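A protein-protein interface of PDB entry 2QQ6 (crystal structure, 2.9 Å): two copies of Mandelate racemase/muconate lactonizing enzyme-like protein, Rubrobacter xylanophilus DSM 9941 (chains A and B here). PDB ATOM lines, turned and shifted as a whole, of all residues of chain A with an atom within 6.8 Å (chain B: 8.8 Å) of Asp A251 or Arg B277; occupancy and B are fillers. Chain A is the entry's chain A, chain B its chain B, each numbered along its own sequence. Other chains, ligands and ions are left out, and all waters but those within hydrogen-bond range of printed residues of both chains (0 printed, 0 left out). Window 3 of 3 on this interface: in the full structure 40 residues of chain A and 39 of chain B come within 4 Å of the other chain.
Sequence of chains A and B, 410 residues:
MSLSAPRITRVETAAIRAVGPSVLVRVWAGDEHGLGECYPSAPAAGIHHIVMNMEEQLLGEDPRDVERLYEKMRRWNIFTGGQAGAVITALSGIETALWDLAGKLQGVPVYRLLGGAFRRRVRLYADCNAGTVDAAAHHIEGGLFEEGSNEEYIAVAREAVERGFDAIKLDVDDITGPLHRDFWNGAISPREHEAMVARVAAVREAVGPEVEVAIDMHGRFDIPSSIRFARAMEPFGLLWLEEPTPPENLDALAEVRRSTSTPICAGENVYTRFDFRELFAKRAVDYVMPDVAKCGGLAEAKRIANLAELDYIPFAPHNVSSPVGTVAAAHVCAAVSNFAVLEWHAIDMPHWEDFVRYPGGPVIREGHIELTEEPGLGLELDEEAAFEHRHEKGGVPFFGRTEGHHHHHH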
ATOM      1  N   ILE A 223     -30.296 -30.137  -2.926  1.00  0.00           N
ATOM      2  CA  ILE A 223     -30.541 -28.730  -3.229  1.00  0.00           C
ATOM      3  C   ILE A 223     -31.982 -28.271  -3.021  1.00  0.00           C
ATOM      4  O   ILE A 223     -32.253 -27.408  -2.193  1.00  0.00           O
ATOM      5  CB  ILE A 223     -30.105 -28.404  -4.691  1.00  0.00           C
ATOM      6  CG1 ILE A 223     -28.574 -28.376  -4.790  1.00  0.00           C
ATOM      7  CG2 ILE A 223     -30.733 -27.102  -5.149  1.00  0.00           C
ATOM      8  CD1 ILE A 223     -27.894 -27.460  -3.800  1.00  0.00           C
ATOM      9  N   GLU A 248     -19.327 -31.943   1.353  1.00  0.00           N
ATOM     10  CA  GLU A 248     -18.312 -31.991   0.316  1.00  0.00           C
ATOM     11  C   GLU A 248     -18.251 -30.888  -0.760  1.00  0.00           C
ATOM     12  O   GLU A 248     -17.171 -30.572  -1.245  1.00  0.00           O
ATOM     13  CB  GLU A 248     -18.281 -33.392  -0.339  1.00  0.00           C
ATOM     14  CG  GLU A 248     -19.593 -34.168  -0.409  1.00  0.00           C
ATOM     15  CD  GLU A 248     -19.950 -34.855   0.892  1.00  0.00           C
ATOM     16  OE1 GLU A 248     -19.028 -35.177   1.664  1.00  0.00           O
ATOM     17  OE2 GLU A 248     -21.148 -35.094   1.139  1.00  0.00           O
ATOM     18  N   ASN A 249     -19.376 -30.296  -1.137  1.00  0.00           N
ATOM     19  CA  ASN A 249     -19.365 -29.245  -2.154  1.00  0.00           C
ATOM     20  C   ASN A 249     -19.827 -27.967  -1.494  1.00  0.00           C
ATOM     21  O   ASN A 249     -20.997 -27.824  -1.144  1.00  0.00           O
ATOM     22  CB  ASN A 249     -20.306 -29.600  -3.311  1.00  0.00           C
ATOM     23  CG  ASN A 249     -20.306 -28.550  -4.428  1.00  0.00           C
ATOM     24  OD1 ASN A 249     -19.947 -27.392  -4.213  1.00  0.00           O
ATOM     25  ND2 ASN A 249     -20.732 -28.959  -5.625  1.00  0.00           N
ATOM     26  N   LEU A 250     -18.902 -27.033  -1.320  1.00  0.00           N
ATOM     27  CA  LEU A 250     -19.230 -25.774  -0.674  1.00  0.00           C
ATOM     28  C   LEU A 250     -20.052 -24.859  -1.570  1.00  0.00           C
ATOM     29  O   LEU A 250     -20.724 -23.957  -1.094  1.00  0.00           O
ATOM     30  CB  LEU A 250     -17.948 -25.071  -0.232  1.00  0.00           C
ATOM     31  CG  LEU A 250     -16.964 -25.934   0.558  1.00  0.00           C
ATOM     32  CD1 LEU A 250     -15.856 -25.061   1.145  1.00  0.00           C
ATOM     33  CD2 LEU A 250     -17.709 -26.663   1.660  1.00  0.00           C
ATOM     34  N   ASP A 251     -19.990 -25.095  -2.872  1.00  0.00           N
ATOM     35  CA  ASP A 251     -20.743 -24.287  -3.817  1.00  0.00           C
ATOM     36  C   ASP A 251     -22.239 -24.442  -3.594  1.00  0.00           C
ATOM     37  O   ASP A 251     -22.993 -23.496  -3.785  1.00  0.00           O
ATOM     38  CB  ASP A 251     -20.394 -24.682  -5.255  1.00  0.00           C
ATOM     39  CG  ASP A 251     -19.060 -24.122  -5.701  1.00  0.00           C
ATOM     40  OD1 ASP A 251     -18.846 -22.910  -5.483  1.00  0.00           O
ATOM     41  OD2 ASP A 251     -18.237 -24.881  -6.271  1.00  0.00           O
ATOM     42  N   ALA A 252     -22.656 -25.635  -3.186  1.00  0.00           N
ATOM     43  CA  ALA A 252     -24.060 -25.927  -2.927  1.00  0.00           C
ATOM     44  C   ALA A 252     -24.575 -25.168  -1.706  1.00  0.00           C
ATOM     45  O   ALA A 252     -25.711 -24.692  -1.671  1.00  0.00           O
ATOM     46  CB  ALA A 252     -24.231 -27.399  -2.720  1.00  0.00           C
ATOM     47  N   LEU A 253     -23.719 -25.067  -0.700  1.00  0.00           N
ATOM     48  CA  LEU A 253     -24.043 -24.361   0.536  1.00  0.00           C
ATOM     49  C   LEU A 253     -24.213 -22.881   0.216  1.00  0.00           C
ATOM     50  O   LEU A 253     -25.104 -22.201   0.720  1.00  0.00           O
ATOM     51  CB  LEU A 253     -22.901 -24.534   1.541  1.00  0.00           C
ATOM     52  CG  LEU A 253     -23.230 -24.175   2.981  1.00  0.00           C
ATOM     53  CD1 LEU A 253     -24.122 -25.254   3.533  1.00  0.00           C
ATOM     54  CD2 LEU A 253     -21.970 -24.048   3.805  1.00  0.00           C
ATOM     55  N   ALA A 254     -23.326 -22.383  -0.622  1.00  0.00           N
ATOM     56  CA  ALA A 254     -23.376 -21.008  -1.017  1.00  0.00           C
ATOM     57  C   ALA A 254     -24.700 -20.766  -1.744  1.00  0.00           C
ATOM     58  O   ALA A 254     -25.389 -19.788  -1.480  1.00  0.00           O
ATOM     59  CB  ALA A 254     -22.215 -20.722  -1.912  1.00  0.00           C
ATOM     60  N   GLU A 255     -25.058 -21.670  -2.649  1.00  0.00           N
ATOM     61  CA  GLU A 255     -26.286 -21.541  -3.420  1.00  0.00           C
ATOM     62  C   GLU A 255     -27.488 -21.513  -2.471  1.00  0.00           C
ATOM     63  O   GLU A 255     -28.470 -20.806  -2.701  1.00  0.00           O
ATOM     64  CB  GLU A 255     -26.399 -22.718  -4.407  1.00  0.00           C
ATOM     65  CG  GLU A 255     -27.263 -22.490  -5.685  1.00  0.00           C
ATOM     66  CD  GLU A 255     -26.652 -21.488  -6.686  1.00  0.00           C
ATOM     67  OE1 GLU A 255     -25.458 -21.124  -6.542  1.00  0.00           O
ATOM     68  OE2 GLU A 255     -27.369 -21.071  -7.629  1.00  0.00           O
ATOM     69  N   VAL A 256     -27.404 -22.290  -1.400  1.00  0.00           N
ATOM     70  CA  VAL A 256     -28.490 -22.339  -0.444  1.00  0.00           C
ATOM     71  C   VAL A 256     -28.504 -21.065   0.357  1.00  0.00           C
ATOM     72  O   VAL A 256     -29.550 -20.447   0.519  1.00  0.00           O
ATOM     73  CB  VAL A 256     -28.357 -23.539   0.532  1.00  0.00           C
ATOM     74  CG1 VAL A 256     -29.446 -23.480   1.583  1.00  0.00           C
ATOM     75  CG2 VAL A 256     -28.472 -24.839  -0.222  1.00  0.00           C
ATOM     76  N   ARG A 258     -27.447 -18.230  -0.367  1.00  0.00           N
ATOM     77  CA  ARG A 258     -27.869 -17.193  -1.294  1.00  0.00           C
ATOM     78  C   ARG A 258     -29.371 -17.221  -1.593  1.00  0.00           C
ATOM     79  O   ARG A 258     -29.918 -16.261  -2.133  1.00  0.00           O
ATOM     80  CB  ARG A 258     -27.069 -17.375  -2.576  1.00  0.00           C
ATOM     81  CG  ARG A 258     -27.258 -16.322  -3.621  1.00  0.00           C
ATOM     82  CD  ARG A 258     -26.479 -16.710  -4.865  1.00  0.00           C
ATOM     83  NE  ARG A 258     -25.078 -16.949  -4.535  1.00  0.00           N
ATOM     84  CZ  ARG A 258     -24.375 -18.004  -4.932  1.00  0.00           C
ATOM     85  NH1 ARG A 258     -24.939 -18.938  -5.691  1.00  0.00           N
ATOM     86  NH2 ARG A 258     -23.107 -18.124  -4.549  1.00  0.00           N
ATOM     87  N   LYS A 282     -16.125 -18.363  -1.205  1.00  0.00           N
ATOM     88  CA  LYS A 282     -17.389 -18.630  -1.854  1.00  0.00           C
ATOM     89  C   LYS A 282     -18.550 -17.985  -1.116  1.00  0.00           C
ATOM     90  O   LYS A 282     -19.701 -18.240  -1.423  1.00  0.00           O
ATOM     91  CB  LYS A 282     -17.608 -20.135  -1.930  1.00  0.00           C
ATOM     92  CG  LYS A 282     -16.502 -20.885  -2.642  1.00  0.00           C
ATOM     93  CD  LYS A 282     -16.795 -22.366  -2.699  1.00  0.00           C
ATOM     94  CE  LYS A 282     -15.812 -23.066  -3.592  1.00  0.00           C
ATOM     95  NZ  LYS A 282     -15.788 -22.410  -4.928  1.00  0.00           N
ATOM     96  N   ALA A 284     -19.877 -18.666   1.475  1.00  0.00           N
ATOM     97  CA  ALA A 284     -20.766 -19.765   1.819  1.00  0.00           C
ATOM     98  C   ALA A 284     -21.470 -19.770   3.165  1.00  0.00           C
ATOM     99  O   ALA A 284     -22.343 -20.602   3.372  1.00  0.00           O
ATOM    100  CB  ALA A 284     -20.028 -21.073   1.645  1.00  0.00           C
ATOM    101  N   LEU B 250      -5.252 -24.810  -4.566  1.00  0.00           N
ATOM    102  CA  LEU B 250      -5.206 -25.162  -5.982  1.00  0.00           C
ATOM    103  C   LEU B 250      -5.149 -23.940  -6.888  1.00  0.00           C
ATOM    104  O   LEU B 250      -4.677 -24.007  -8.027  1.00  0.00           O
ATOM    105  CB  LEU B 250      -6.395 -26.041  -6.348  1.00  0.00           C
ATOM    106  CG  LEU B 250      -6.477 -27.328  -5.533  1.00  0.00           C
ATOM    107  CD1 LEU B 250      -7.414 -28.289  -6.215  1.00  0.00           C
ATOM    108  CD2 LEU B 250      -5.113 -27.951  -5.393  1.00  0.00           C
ATOM    109  N   VAL B 270      -5.113 -35.162  -3.528  1.00  0.00           N
ATOM    110  CA  VAL B 270      -6.506 -34.749  -3.470  1.00  0.00           C
ATOM    111  C   VAL B 270      -7.368 -36.011  -3.479  1.00  0.00           C
ATOM    112  O   VAL B 270      -7.134 -36.911  -4.285  1.00  0.00           O
ATOM    113  CB  VAL B 270      -6.855 -33.826  -4.666  1.00  0.00           C
ATOM    114  CG1 VAL B 270      -6.180 -34.326  -5.924  1.00  0.00           C
ATOM    115  CG2 VAL B 270      -8.357 -33.767  -4.865  1.00  0.00           C
ATOM    116  N   TYR B 271      -8.343 -36.087  -2.572  1.00  0.00           N
ATOM    117  CA  TYR B 271      -9.213 -37.262  -2.482  1.00  0.00           C
ATOM    118  C   TYR B 271     -10.649 -36.963  -2.905  1.00  0.00           C
ATOM    119  O   TYR B 271     -11.101 -35.827  -2.811  1.00  0.00           O
ATOM    120  CB  TYR B 271      -9.273 -37.784  -1.044  1.00  0.00           C
ATOM    121  CG  TYR B 271      -7.963 -37.902  -0.303  1.00  0.00           C
ATOM    122  CD1 TYR B 271      -7.188 -36.781  -0.030  1.00  0.00           C
ATOM    123  CD2 TYR B 271      -7.517 -39.144   0.164  1.00  0.00           C
ATOM    124  CE1 TYR B 271      -6.001 -36.890   0.694  1.00  0.00           C
ATOM    125  CE2 TYR B 271      -6.332 -39.265   0.888  1.00  0.00           C
ATOM    126  CZ  TYR B 271      -5.579 -38.134   1.151  1.00  0.00           C
ATOM    127  OH  TYR B 271      -4.415 -38.235   1.880  1.00  0.00           O
ATOM    128  N   THR B 272     -11.363 -37.995  -3.346  1.00  0.00           N
ATOM    129  CA  THR B 272     -12.781 -37.907  -3.753  1.00  0.00           C
ATOM    130  C   THR B 272     -13.160 -37.058  -4.949  1.00  0.00           C
ATOM    131  O   THR B 272     -12.545 -36.034  -5.251  1.00  0.00           O
ATOM    132  CB  THR B 272     -13.733 -37.443  -2.600  1.00  0.00           C
ATOM    133  OG1 THR B 272     -13.469 -36.077  -2.267  1.00  0.00           O
ATOM    134  CG2 THR B 272     -13.565 -38.313  -1.376  1.00  0.00           C
ATOM    135  N   ARG B 273     -14.222 -37.496  -5.607  1.00  0.00           N
ATOM    136  CA  ARG B 273     -14.731 -36.816  -6.775  1.00  0.00           C
ATOM    137  C   ARG B 273     -15.034 -35.356  -6.465  1.00  0.00           C
ATOM    138  O   ARG B 273     -14.784 -34.473  -7.283  1.00  0.00           O
ATOM    139  CB  ARG B 273     -15.989 -37.523  -7.265  1.00  0.00           C
ATOM    140  CG  ARG B 273     -17.031 -37.746  -6.190  1.00  0.00           C
ATOM    141  CD  ARG B 273     -18.264 -38.361  -6.817  1.00  0.00           C
ATOM    142  NE  ARG B 273     -19.286 -38.699  -5.834  1.00  0.00           N
ATOM    143  CZ  ARG B 273     -19.191 -39.696  -4.962  1.00  0.00           C
ATOM    144  NH1 ARG B 273     -18.117 -40.471  -4.940  1.00  0.00           N
ATOM    145  NH2 ARG B 273     -20.176 -39.912  -4.108  1.00  0.00           N
ATOM    146  N   PHE B 274     -15.569 -35.100  -5.282  1.00  0.00           N
ATOM    147  CA  PHE B 274     -15.887 -33.739  -4.895  1.00  0.00           C
ATOM    148  C   PHE B 274     -14.697 -32.792  -4.960  1.00  0.00           C
ATOM    149  O   PHE B 274     -14.847 -31.615  -5.272  1.00  0.00           O
ATOM    150  CB  PHE B 274     -16.474 -33.730  -3.492  1.00  0.00           C
ATOM    151  CG  PHE B 274     -17.782 -34.447  -3.394  1.00  0.00           C
ATOM    152  CD1 PHE B 274     -17.851 -35.732  -2.853  1.00  0.00           C
ATOM    153  CD2 PHE B 274     -18.951 -33.851  -3.876  1.00  0.00           C
ATOM    154  CE1 PHE B 274     -19.071 -36.415  -2.791  1.00  0.00           C
ATOM    155  CE2 PHE B 274     -20.174 -34.521  -3.822  1.00  0.00           C
ATOM    156  CZ  PHE B 274     -20.238 -35.803  -3.280  1.00  0.00           C
ATOM    157  N   ASP B 275     -13.509 -33.299  -4.673  1.00  0.00           N
ATOM    158  CA  ASP B 275     -12.339 -32.449  -4.701  1.00  0.00           C
ATOM    159  C   ASP B 275     -11.711 -32.321  -6.078  1.00  0.00           C
ATOM    160  O   ASP B 275     -11.125 -31.295  -6.406  1.00  0.00           O
ATOM    161  CB  ASP B 275     -11.323 -32.942  -3.682  1.00  0.00           C
ATOM    162  CG  ASP B 275     -11.846 -32.853  -2.261  1.00  0.00           C
ATOM    163  OD1 ASP B 275     -12.218 -31.743  -1.822  1.00  0.00           O
ATOM    164  OD2 ASP B 275     -11.890 -33.895  -1.581  1.00  0.00           O
ATOM    165  N   PHE B 276     -11.827 -33.352  -6.896  1.00  0.00           N
ATOM    166  CA  PHE B 276     -11.269 -33.252  -8.231  1.00  0.00           C
ATOM    167  C   PHE B 276     -12.149 -32.330  -9.061  1.00  0.00           C
ATOM    168  O   PHE B 276     -11.699 -31.736 -10.042  1.00  0.00           O
ATOM    169  CB  PHE B 276     -11.157 -34.632  -8.885  1.00  0.00           C
ATOM    170  CG  PHE B 276      -9.900 -35.356  -8.526  1.00  0.00           C
ATOM    171  CD1 PHE B 276      -9.789 -36.026  -7.316  1.00  0.00           C
ATOM    172  CD2 PHE B 276      -8.794 -35.311  -9.370  1.00  0.00           C
ATOM    173  CE1 PHE B 276      -8.591 -36.633  -6.942  1.00  0.00           C
ATOM    174  CE2 PHE B 276      -7.586 -35.911  -9.008  1.00  0.00           C
ATOM    175  CZ  PHE B 276      -7.488 -36.575  -7.793  1.00  0.00           C
ATOM    176  N   ARG B 277     -13.408 -32.212  -8.659  1.00  0.00           N
ATOM    177  CA  ARG B 277     -14.339 -31.332  -9.347  1.00  0.00           C
ATOM    178  C   ARG B 277     -13.779 -29.924  -9.287  1.00  0.00           C
ATOM    179  O   ARG B 277     -13.653 -29.248 -10.307  1.00  0.00           O
ATOM    180  CB  ARG B 277     -15.710 -31.355  -8.678  1.00  0.00           C
ATOM    181  CG  ARG B 277     -16.510 -30.114  -8.969  1.00  0.00           C
ATOM    182  CD  ARG B 277     -17.980 -30.310  -8.727  1.00  0.00           C
ATOM    183  NE  ARG B 277     -18.722 -29.068  -8.942  1.00  0.00           N
ATOM    184  CZ  ARG B 277     -18.744 -28.045  -8.086  1.00  0.00           C
ATOM    185  NH1 ARG B 277     -18.061 -28.103  -6.940  1.00  0.00           N
ATOM    186  NH2 ARG B 277     -19.462 -26.966  -8.370  1.00  0.00           N
ATOM    187  N   GLU B 278     -13.448 -29.491  -8.076  1.00  0.00           N
ATOM    188  CA  GLU B 278     -12.877 -28.174  -7.854  1.00  0.00           C
ATOM    189  C   GLU B 278     -11.575 -28.034  -8.627  1.00  0.00           C
ATOM    190  O   GLU B 278     -11.282 -26.983  -9.181  1.00  0.00           O
ATOM    191  CB  GLU B 278     -12.628 -27.975  -6.366  1.00  0.00           C
ATOM    192  CG  GLU B 278     -13.901 -27.848  -5.538  1.00  0.00           C
ATOM    193  CD  GLU B 278     -14.563 -26.469  -5.665  1.00  0.00           C
ATOM    194  OE1 GLU B 278     -15.663 -26.277  -5.091  1.00  0.00           O
ATOM    195  OE2 GLU B 278     -13.983 -25.579  -6.328  1.00  0.00           O
ATOM    196  N   LEU B 279     -10.792 -29.105  -8.667  1.00  0.00           N
ATOM    197  CA  LEU B 279      -9.534 -29.084  -9.394  1.00  0.00           C
ATOM    198  C   LEU B 279      -9.818 -28.720 -10.849  1.00  0.00           C
ATOM    199  O   LEU B 279      -9.385 -27.680 -11.340  1.00  0.00           O
ATOM    200  CB  LEU B 279      -8.861 -30.453  -9.338  1.00  0.00           C
ATOM    201  CG  LEU B 279      -7.407 -30.476  -9.804  1.00  0.00           C
ATOM    202  CD1 LEU B 279      -6.534 -29.834  -8.758  1.00  0.00           C
ATOM    203  CD2 LEU B 279      -6.963 -31.895 -10.042  1.00  0.00           C
ATOM    204  N   PHE B 280     -10.556 -29.586 -11.531  1.00  0.00           N
ATOM    205  CA  PHE B 280     -10.904 -29.354 -12.921  1.00  0.00           C
ATOM    206  C   PHE B 280     -11.605 -28.024 -13.086  1.00  0.00           C
ATOM    207  O   PHE B 280     -11.461 -27.370 -14.109  1.00  0.00           O
ATOM    208  CB  PHE B 280     -11.777 -30.497 -13.429  1.00  0.00           C
ATOM    209  CG  PHE B 280     -11.083 -31.818 -13.404  1.00  0.00           C
ATOM    210  CD1 PHE B 280     -11.673 -32.922 -12.799  1.00  0.00           C
ATOM    211  CD2 PHE B 280      -9.802 -31.943 -13.933  1.00  0.00           C
ATOM    212  CE1 PHE B 280     -10.989 -34.133 -12.719  1.00  0.00           C
ATOM    213  CE2 PHE B 280      -9.118 -33.139 -13.858  1.00  0.00           C
ATOM    214  CZ  PHE B 280      -9.709 -34.237 -13.250  1.00  0.00           C
ATOM    215  N   ALA B 281     -12.352 -27.617 -12.069  1.00  0.00           N
ATOM    216  CA  ALA B 281     -13.057 -26.337 -12.108  1.00  0.00           C
ATOM    217  C   ALA B 281     -12.075 -25.182 -12.319  1.00  0.00           C
ATOM    218  O   ALA B 281     -12.277 -24.339 -13.196  1.00  0.00           O
ATOM    219  CB  ALA B 281     -13.838 -26.121 -10.820  1.00  0.00           C
ATOM    220  N   LYS B 282     -11.016 -25.151 -11.511  1.00  0.00           N
ATOM    221  CA  LYS B 282     -10.006 -24.110 -11.618  1.00  0.00           C
ATOM    222  C   LYS B 282      -9.118 -24.252 -12.851  1.00  0.00           C
ATOM    223  O   LYS B 282      -8.304 -23.380 -13.118  1.00  0.00           O
ATOM    224  CB  LYS B 282      -9.111 -24.100 -10.382  1.00  0.00           C
ATOM    225  CG  LYS B 282      -9.696 -23.439  -9.147  1.00  0.00           C
ATOM    226  CD  LYS B 282     -10.358 -24.434  -8.217  1.00  0.00           C
ATOM    227  CE  LYS B 282     -10.295 -23.956  -6.775  1.00  0.00           C
ATOM    228  NZ  LYS B 282     -10.832 -22.580  -6.624  1.00  0.00           N
ATOM    229  N   ARG B 283      -9.274 -25.339 -13.601  1.00  0.00           N
ATOM    230  CA  ARG B 283      -8.448 -25.579 -14.784  1.00  0.00           C
ATOM    231  C   ARG B 283      -6.974 -25.527 -14.356  1.00  0.00           C
ATOM    232  O   ARG B 283      -6.167 -24.803 -14.951  1.00  0.00           O
ATOM    233  CB  ARG B 283      -8.678 -24.493 -15.842  1.00  0.00           C
ATOM    234  CG  ARG B 283     -10.109 -24.238 -16.265  1.00  0.00           C
ATOM    235  CD  ARG B 283     -10.177 -22.910 -17.030  1.00  0.00           C
ATOM    236  NE  ARG B 283      -9.481 -21.838 -16.303  1.00  0.00           N
ATOM    237  CZ  ARG B 283      -9.435 -20.554 -16.671  1.00  0.00           C
ATOM    238  NH1 ARG B 283     -10.051 -20.136 -17.778  1.00  0.00           N
ATOM    239  NH2 ARG B 283      -8.759 -19.678 -15.926  1.00  0.00           N
ATOM    240  N   ALA B 284      -6.619 -26.305 -13.337  1.00  0.00           N
ATOM    241  CA  ALA B 284      -5.259 -26.283 -12.809  1.00  0.00           C
ATOM    242  C   ALA B 284      -4.286 -27.336 -13.308  1.00  0.00           C
ATOM    243  O   ALA B 284      -3.104 -27.254 -13.010  1.00  0.00           O
ATOM    244  CB  ALA B 284      -5.315 -26.333 -11.287  1.00  0.00           C
ATOM    245  N   VAL B 288      -3.918 -35.434 -14.761  1.00  0.00           N
ATOM    246  CA  VAL B 288      -4.479 -35.726 -13.450  1.00  0.00           C
ATOM    247  C   VAL B 288      -3.888 -37.034 -13.009  1.00  0.00           C
ATOM    248  O   VAL B 288      -3.680 -37.925 -13.830  1.00  0.00           O
ATOM    249  CB  VAL B 288      -5.988 -35.928 -13.488  1.00  0.00           C
ATOM    250  CG1 VAL B 288      -6.571 -35.530 -12.165  1.00  0.00           C
ATOM    251  CG2 VAL B 288      -6.598 -35.145 -14.613  1.00  0.00           C
ATOM    252  N   ARG B 303     -14.695 -42.448 -11.858  1.00  0.00           N
ATOM    253  CA  ARG B 303     -15.483 -41.222 -11.914  1.00  0.00           C
ATOM    254  C   ARG B 303     -14.510 -40.068 -12.165  1.00  0.00           C
ATOM    255  O   ARG B 303     -14.730 -39.225 -13.039  1.00  0.00           O
ATOM    256  CB  ARG B 303     -16.214 -40.973 -10.582  1.00  0.00           C
ATOM    257  CG  ARG B 303     -17.632 -41.542 -10.464  1.00  0.00           C
ATOM    258  CD  ARG B 303     -18.592 -40.453  -9.999  1.00  0.00           C
ATOM    259  NE  ARG B 303     -19.683 -40.952  -9.156  1.00  0.00           N
ATOM    260  CZ  ARG B 303     -20.608 -40.178  -8.578  1.00  0.00           C
ATOM    261  NH1 ARG B 303     -20.599 -38.856  -8.740  1.00  0.00           N
ATOM    262  NH2 ARG B 303     -21.551 -40.731  -7.832  1.00  0.00           N
ATOM    263  N   ILE B 304     -13.434 -40.039 -11.382  1.00  0.00           N
ATOM    264  CA  ILE B 304     -12.413 -39.004 -11.504  1.00  0.00           C
ATOM    265  C   ILE B 304     -11.894 -38.890 -12.933  1.00  0.00           C
ATOM    266  O   ILE B 304     -11.750 -37.785 -13.457  1.00  0.00           O
ATOM    267  CB  ILE B 304     -11.239 -39.275 -10.533  1.00  0.00           C
ATOM    268  CG1 ILE B 304     -11.713 -39.031  -9.095  1.00  0.00           C
ATOM    269  CG2 ILE B 304     -10.036 -38.400 -10.891  1.00  0.00           C
ATOM    270  CD1 ILE B 304     -10.655 -39.207  -8.037  1.00  0.00           C
ATOM    271  N   LEU B 307     -14.491 -37.300 -15.210  1.00  0.00           N
ATOM    272  CA  LEU B 307     -14.605 -35.857 -15.056  1.00  0.00           C
ATOM    273  C   LEU B 307     -13.583 -35.185 -15.940  1.00  0.00           C
ATOM    274  O   LEU B 307     -13.893 -34.232 -16.643  1.00  0.00           O
ATOM    275  CB  LEU B 307     -14.396 -35.441 -13.603  1.00  0.00           C
ATOM    276  CG  LEU B 307     -15.609 -35.562 -12.665  1.00  0.00           C
ATOM    277  CD1 LEU B 307     -15.242 -34.989 -11.296  1.00  0.00           C
ATOM    278  CD2 LEU B 307     -16.815 -34.814 -13.237  1.00  0.00           C
ATOM    279  N   ALA B 308     -12.365 -35.711 -15.909  1.00  0.00           N
ATOM    280  CA  ALA B 308     -11.264 -35.192 -16.715  1.00  0.00           C
ATOM    281  C   ALA B 308     -11.510 -35.400 -18.211  1.00  0.00           C
ATOM    282  O   ALA B 308     -11.138 -34.565 -19.033  1.00  0.00           O
ATOM    283  CB  ALA B 308      -9.971 -35.874 -16.303  1.00  0.00           C
ATOM    284  N   ASP B 311     -13.009 -32.695 -19.991  1.00  0.00           N
ATOM    285  CA  ASP B 311     -12.126 -31.605 -20.393  1.00  0.00           C
ATOM    286  C   ASP B 311     -10.959 -31.980 -21.288  1.00  0.00           C
ATOM    287  O   ASP B 311     -10.076 -31.164 -21.509  1.00  0.00           O
ATOM    288  CB  ASP B 311     -11.597 -30.883 -19.159  1.00  0.00           C
ATOM    289  CG  ASP B 311     -12.490 -29.746 -18.723  1.00  0.00           C
ATOM    290  OD1 ASP B 311     -12.524 -28.710 -19.431  1.00  0.00           O
ATOM    291  OD2 ASP B 311     -13.160 -29.896 -17.675  1.00  0.00           O
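The guanidinium group of Arg B277 sits close to the side-chain amide nitrogen of Asn A249, 3.1 Å away. The side-chain carboxylate (OD2) of Asp A251 lies within salt-bridge range of the guanidinium group (NH2) of Arg B277 (3.2 Å). NZ of Lys A282 is in salt-bridge range of OE1 of Glu B278. The side-chain carboxylate of Asp A251 sits close to the side-chain carboxylate of Glu B278 (3.2 Å).
OD1 of Asn A249 is in hydrogen-bond range of N of Asp A251 (2.7 Å). The side-chain amide oxygen (OD1) of Asn A249 is in hydrogen-bond range of the backbone NH (N) of Ala A252 (3.4 Å). OD1 of Asp A251 is in salt-bridge range of NZ of Lys A282, 3.1 Å away. NH1 of Arg B277 is in salt-bridge range of OE1 of Glu B278 (3.5 Å).
Phe B274 touches Glu A248.
Of chain B, only Arg B277 (3.2 Å) and Glu B278 (3.2 Å) come within 4 Å of Asp A251. Arg B277 touches two residues of chain A. No residue of chain B comes within 4 Å of Ala A252. Of the printed residues of chain A, Glu B278 touches Asp A251 (3.2 Å) and Lys A282 (3.5 Å). Printed residues of chain B within 4 Å of Asn A249: Arg B277 (3.1 Å). Arg B283 touches none of the printed residues of chain A. Leu B279 touches none of the printed residues of chain A. The nearest residue of chain B that does not touch Asp A251 is Ala B281 (6.4 Å). The nearest residue of chain A that does not touch Arg B277 is Leu A250 (5.8 Å). The nearest printed residue of chain B that does not touch Glu A248 is Asp B275 (5.1 Å).
Printed residues of chain A that touch a printed residue of chain B: Glu A248, Asn A249, Asp A251 and Lys A282. Of the 22 printed residues of chain B, 3 touch a printed residue of chain A. Hydrophobic or aromatic side chains of chain B that line the printed part of chain A: Phe B274. Among the printed residues, 5 pairs touch across the chains. Among the printed residues, Asp or Glu carboxylates within 4 Å of a Lys or Arg side-chain nitrogen of the other chain: Asp A251 with Arg B277 and Lys A282 with Glu B278.
Positions printed for both chains: 250, 282 and 284. Of the 5 pairs that touch across the chains among the printed residues, none has its exchanged pair printed and touching as well.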
